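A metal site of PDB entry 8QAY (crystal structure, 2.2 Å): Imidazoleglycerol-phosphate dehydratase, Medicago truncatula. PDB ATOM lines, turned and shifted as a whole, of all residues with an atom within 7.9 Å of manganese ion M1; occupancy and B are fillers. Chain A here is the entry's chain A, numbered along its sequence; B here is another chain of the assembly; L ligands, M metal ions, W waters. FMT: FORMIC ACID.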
ATOM      1  N   PHE A  43       3.265  -0.558 -26.761  1.00  0.00           N
ATOM      2  CA  PHE A  43       3.665  -1.821 -26.153  1.00  0.00           C
ATOM      3  C   PHE A  43       5.051  -2.232 -26.644  1.00  0.00           C
ATOM      4  O   PHE A  43       5.861  -2.724 -25.852  1.00  0.00           O
ATOM      5  CB  PHE A  43       2.656  -2.952 -26.433  1.00  0.00           C
ATOM      6  CG  PHE A  43       2.953  -4.184 -25.637  1.00  0.00           C
ATOM      7  CD1 PHE A  43       2.531  -4.286 -24.314  1.00  0.00           C
ATOM      8  CD2 PHE A  43       3.734  -5.202 -26.162  1.00  0.00           C
ATOM      9  CE1 PHE A  43       2.849  -5.404 -23.544  1.00  0.00           C
ATOM     10  CE2 PHE A  43       4.042  -6.332 -25.398  1.00  0.00           C
ATOM     11  CZ  PHE A  43       3.613  -6.419 -24.076  1.00  0.00           C
ATOM     12  N   HIS A  46       7.653  -0.360 -24.658  1.00  0.00           N
ATOM     13  CA  HIS A  46       7.865  -1.037 -23.386  1.00  0.00           C
ATOM     14  C   HIS A  46       8.805  -2.235 -23.547  1.00  0.00           C
ATOM     15  O   HIS A  46       9.715  -2.427 -22.738  1.00  0.00           O
ATOM     16  CB  HIS A  46       6.496  -1.444 -22.815  1.00  0.00           C
ATOM     17  CG  HIS A  46       6.547  -2.095 -21.474  1.00  0.00           C
ATOM     18  ND1 HIS A  46       7.364  -1.664 -20.460  1.00  0.00           N
ATOM     19  CD2 HIS A  46       5.855  -3.147 -20.978  1.00  0.00           C
ATOM     20  CE1 HIS A  46       7.176  -2.418 -19.390  1.00  0.00           C
ATOM     21  NE2 HIS A  46       6.268  -3.329 -19.684  1.00  0.00           N
ATOM     22  N   MET A  47       8.636  -3.007 -24.626  1.00  0.00           N
ATOM     23  CA  MET A  47       9.512  -4.164 -24.851  1.00  0.00           C
ATOM     24  C   MET A  47      10.915  -3.728 -25.241  1.00  0.00           C
ATOM     25  O   MET A  47      11.904  -4.326 -24.787  1.00  0.00           O
ATOM     26  CB  MET A  47       8.921  -5.088 -25.917  1.00  0.00           C
ATOM     27  CG  MET A  47       7.598  -5.757 -25.523  1.00  0.00           C
ATOM     28  SD  MET A  47       7.725  -6.788 -24.032  1.00  0.00           S
ATOM     29  CE  MET A  47       7.197  -5.646 -22.746  1.00  0.00           C
ATOM     30  N   GLN A  50      12.840  -2.948 -22.224  1.00  0.00           N
ATOM     31  CA  GLN A  50      13.405  -4.143 -21.586  1.00  0.00           C
ATOM     32  C   GLN A  50      14.726  -4.533 -22.217  1.00  0.00           C
ATOM     33  O   GLN A  50      15.641  -5.010 -21.530  1.00  0.00           O
ATOM     34  CB  GLN A  50      12.428  -5.306 -21.704  1.00  0.00           C
ATOM     35  CG  GLN A  50      11.080  -5.023 -21.106  1.00  0.00           C
ATOM     36  CD  GLN A  50      11.196  -4.748 -19.642  1.00  0.00           C
ATOM     37  OE1 GLN A  50      11.822  -5.509 -18.918  1.00  0.00           O
ATOM     38  NE2 GLN A  50      10.610  -3.653 -19.200  1.00  0.00           N
ATOM     39  N   LEU A 106       8.804 -14.683 -15.691  1.00  0.00           N
ATOM     40  CA  LEU A 106       8.042 -13.510 -15.249  1.00  0.00           C
ATOM     41  C   LEU A 106       6.753 -14.069 -14.642  1.00  0.00           C
ATOM     42  O   LEU A 106       5.821 -14.448 -15.360  1.00  0.00           O
ATOM     43  CB  LEU A 106       7.760 -12.529 -16.394  1.00  0.00           C
ATOM     44  CG  LEU A 106       7.452 -11.067 -16.003  1.00  0.00           C
ATOM     45  CD1 LEU A 106       7.171 -10.220 -17.229  1.00  0.00           C
ATOM     46  CD2 LEU A 106       6.275 -10.926 -15.053  1.00  0.00           C
ATOM     47  N   HIS A 168       0.836 -10.553 -21.778  1.00  0.00           N
ATOM     48  CA  HIS A 168       1.826  -9.531 -21.424  1.00  0.00           C
ATOM     49  C   HIS A 168       3.046 -10.171 -20.762  1.00  0.00           C
ATOM     50  O   HIS A 168       4.194  -9.836 -21.096  1.00  0.00           O
ATOM     51  CB  HIS A 168       1.150  -8.509 -20.496  1.00  0.00           C
ATOM     52  CG  HIS A 168       1.976  -7.293 -20.171  1.00  0.00           C
ATOM     53  ND1 HIS A 168       1.445  -6.023 -20.148  1.00  0.00           N
ATOM     54  CD2 HIS A 168       3.273  -7.167 -19.816  1.00  0.00           C
ATOM     55  CE1 HIS A 168       2.380  -5.160 -19.810  1.00  0.00           C
ATOM     56  NE2 HIS A 168       3.505  -5.829 -19.607  1.00  0.00           N
ATOM     57  N   HIS A 169       2.825 -11.108 -19.838  1.00  0.00           N
ATOM     58  CA  HIS A 169       3.939 -11.771 -19.169  1.00  0.00           C
ATOM     59  C   HIS A 169       4.787 -12.577 -20.148  1.00  0.00           C
ATOM     60  O   HIS A 169       6.027 -12.539 -20.093  1.00  0.00           O
ATOM     61  CB  HIS A 169       3.409 -12.693 -18.075  1.00  0.00           C
ATOM     62  CG  HIS A 169       2.924 -11.970 -16.877  1.00  0.00           C
ATOM     63  ND1 HIS A 169       2.363 -12.617 -15.803  1.00  0.00           N
ATOM     64  CD2 HIS A 169       2.923 -10.650 -16.578  1.00  0.00           C
ATOM     65  CE1 HIS A 169       2.043 -11.730 -14.878  1.00  0.00           C
ATOM     66  NE2 HIS A 169       2.372 -10.537 -15.326  1.00  0.00           N
ATOM     67  N   GLU A 172       6.788 -10.189 -22.430  1.00  0.00           N
ATOM     68  CA  GLU A 172       7.844  -9.492 -21.713  1.00  0.00           C
ATOM     69  C   GLU A 172       8.951 -10.448 -21.292  1.00  0.00           C
ATOM     70  O   GLU A 172      10.141 -10.130 -21.433  1.00  0.00           O
ATOM     71  CB  GLU A 172       7.255  -8.751 -20.499  1.00  0.00           C
ATOM     72  CG  GLU A 172       8.239  -7.753 -19.873  1.00  0.00           C
ATOM     73  CD  GLU A 172       7.627  -6.900 -18.762  1.00  0.00           C
ATOM     74  OE1 GLU A 172       6.485  -6.426 -18.929  1.00  0.00           O
ATOM     75  OE2 GLU A 172       8.294  -6.701 -17.729  1.00  0.00           O
ATOM     76  N   LYS A 176      12.921 -10.093 -22.069  1.00  0.00           N
ATOM     77  CA  LYS A 176      13.938 -10.143 -21.022  1.00  0.00           C
ATOM     78  C   LYS A 176      14.996 -11.200 -21.338  1.00  0.00           C
ATOM     79  O   LYS A 176      16.197 -10.916 -21.297  1.00  0.00           O
ATOM     80  CB  LYS A 176      13.301 -10.457 -19.652  1.00  0.00           C
ATOM     81  CG  LYS A 176      12.447  -9.365 -19.038  1.00  0.00           C
ATOM     82  CD  LYS A 176      11.910  -9.846 -17.706  1.00  0.00           C
ATOM     83  CE  LYS A 176      10.660  -9.099 -17.238  1.00  0.00           C
ATOM     84  NZ  LYS A 176      10.939  -7.771 -16.672  1.00  0.00           N
ATOM     85  N   GLU B  20       5.812   3.617 -13.555  1.00  0.00           N
ATOM     86  CA  GLU B  20       4.690   3.165 -14.372  1.00  0.00           C
ATOM     87  C   GLU B  20       3.347   3.633 -13.857  1.00  0.00           C
ATOM     88  O   GLU B  20       2.440   3.880 -14.654  1.00  0.00           O
ATOM     89  CB  GLU B  20       4.689   1.627 -14.409  1.00  0.00           C
ATOM     90  CG  GLU B  20       5.893   0.979 -15.081  1.00  0.00           C
ATOM     91  CD  GLU B  20       7.090   0.844 -14.169  1.00  0.00           C
ATOM     92  OE1 GLU B  20       6.936   1.049 -12.946  1.00  0.00           O
ATOM     93  OE2 GLU B  20       8.182   0.495 -14.673  1.00  0.00           O
ATOM     94  N   ASP B  66       0.493   4.040 -16.790  1.00  0.00           N
ATOM     95  CA  ASP B  66       0.835   3.978 -18.198  1.00  0.00           C
ATOM     96  C   ASP B  66      -0.210   3.192 -18.974  1.00  0.00           C
ATOM     97  O   ASP B  66       0.120   2.258 -19.720  1.00  0.00           O
ATOM     98  CB  ASP B  66       2.243   3.383 -18.393  1.00  0.00           C
ATOM     99  CG  ASP B  66       2.412   2.031 -17.730  1.00  0.00           C
ATOM    100  OD1 ASP B  66       1.420   1.457 -17.221  1.00  0.00           O
ATOM    101  OD2 ASP B  66       3.551   1.498 -17.750  1.00  0.00           O
ATOM    102  N   ILE B  69       0.117   1.932 -22.598  1.00  0.00           N
ATOM    103  CA  ILE B  69       0.729   0.656 -22.950  1.00  0.00           C
ATOM    104  C   ILE B  69      -0.374  -0.390 -22.965  1.00  0.00           C
ATOM    105  O   ILE B  69      -0.702  -0.942 -24.025  1.00  0.00           O
ATOM    106  CB  ILE B  69       1.869   0.280 -21.983  1.00  0.00           C
ATOM    107  CG1 ILE B  69       3.067   1.198 -22.176  1.00  0.00           C
ATOM    108  CG2 ILE B  69       2.287  -1.176 -22.175  1.00  0.00           C
ATOM    109  CD1 ILE B  69       4.099   1.060 -21.098  1.00  0.00           C
ATOM    110  N   ASP B  70      -0.928  -0.667 -21.787  1.00  0.00           N
ATOM    111  CA  ASP B  70      -2.173  -1.400 -21.590  1.00  0.00           C
ATOM    112  C   ASP B  70      -2.553  -1.211 -20.121  1.00  0.00           C
ATOM    113  O   ASP B  70      -1.887  -0.455 -19.408  1.00  0.00           O
ATOM    114  CB  ASP B  70      -2.066  -2.877 -22.010  1.00  0.00           C
ATOM    115  CG  ASP B  70      -1.139  -3.698 -21.118  1.00  0.00           C
ATOM    116  OD1 ASP B  70      -0.481  -3.124 -20.235  1.00  0.00           O
ATOM    117  OD2 ASP B  70      -1.094  -4.936 -21.285  1.00  0.00           O
ATOM    118  N   HIS B  72      -2.349  -3.312 -17.704  1.00  0.00           N
ATOM    119  CA  HIS B  72      -1.743  -4.347 -16.849  1.00  0.00           C
ATOM    120  C   HIS B  72      -1.075  -3.744 -15.613  1.00  0.00           C
ATOM    121  O   HIS B  72      -1.327  -4.183 -14.501  1.00  0.00           O
ATOM    122  CB  HIS B  72      -0.734  -5.157 -17.670  1.00  0.00           C
ATOM    123  CG  HIS B  72      -0.165  -6.351 -16.942  1.00  0.00           C
ATOM    124  ND1 HIS B  72      -0.320  -7.646 -17.401  1.00  0.00           N
ATOM    125  CD2 HIS B  72       0.589  -6.440 -15.824  1.00  0.00           C
ATOM    126  CE1 HIS B  72       0.307  -8.478 -16.586  1.00  0.00           C
ATOM    127  NE2 HIS B  72       0.860  -7.770 -15.618  1.00  0.00           N
ATOM    128  N   HIS B  73      -0.178  -2.767 -15.807  1.00  0.00           N
ATOM    129  CA  HIS B  73       0.588  -2.225 -14.686  1.00  0.00           C
ATOM    130  C   HIS B  73      -0.318  -1.537 -13.677  1.00  0.00           C
ATOM    131  O   HIS B  73      -0.175  -1.759 -12.467  1.00  0.00           O
ATOM    132  CB  HIS B  73       1.657  -1.258 -15.189  1.00  0.00           C
ATOM    133  CG  HIS B  73       2.671  -1.883 -16.093  1.00  0.00           C
ATOM    134  ND1 HIS B  73       3.412  -1.152 -16.992  1.00  0.00           N
ATOM    135  CD2 HIS B  73       3.072  -3.176 -16.232  1.00  0.00           C
ATOM    136  CE1 HIS B  73       4.227  -1.954 -17.651  1.00  0.00           C
ATOM    137  NE2 HIS B  73       4.029  -3.184 -17.210  1.00  0.00           N
ATOM    138  N   GLU B  76      -2.320  -4.257 -11.768  1.00  0.00           N
ATOM    139  CA  GLU B  76      -1.480  -4.963 -10.810  1.00  0.00           C
ATOM    140  C   GLU B  76      -1.163  -4.080  -9.597  1.00  0.00           C
ATOM    141  O   GLU B  76      -1.329  -4.511  -8.450  1.00  0.00           O
ATOM    142  CB  GLU B  76      -0.183  -5.422 -11.513  1.00  0.00           C
ATOM    143  CG  GLU B  76       0.850  -6.125 -10.635  1.00  0.00           C
ATOM    144  CD  GLU B  76       1.882  -6.928 -11.428  1.00  0.00           C
ATOM    145  OE1 GLU B  76       1.835  -6.900 -12.682  1.00  0.00           O
ATOM    146  OE2 GLU B  76       2.723  -7.624 -10.810  1.00  0.00           O
HETATM  147  C   FMT L   1       3.969  -6.651 -16.236  1.00  0.00           C
HETATM  148  O1  FMT L   1       3.791  -7.316 -15.177  1.00  0.00           O
HETATM  149  O2  FMT L   1       5.075  -6.071 -16.481  1.00  0.00           O
HETATM  150 MN    MN M   1       5.217  -4.859 -18.223  1.00  0.00          MN
HETATM  151 MN    MN M   2       2.217  -8.613 -13.993  1.00  0.00          MN
HETATM  152  O   HOH W   1       7.053  -4.340 -16.942  1.00  0.00           O
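The side-chain carboxylate (OE2) of Glu 172 lies within salt-bridge range of the side-chain amino group (NZ) of Lys 176 (3.0 Å). A ring nitrogen (ND1) of His 73 of chain B sits at hydrogen-bond distance from the side-chain carboxylate (OD2) of Asp 66 of chain B. OD2 of Asp 70 of chain B sits at hydrogen-bond distance from ND1 of His 168.
Manganese ion M1 is bound by O2 of the ligand (2.1 Å), OE1 of Glu 172 (2.1 Å), NE2 of His 73 of chain B (2.3 Å), water W1 (2.3 Å), NE2 of His 46 (2.4 Å) and NE2 of His 168 (2.4 Å).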
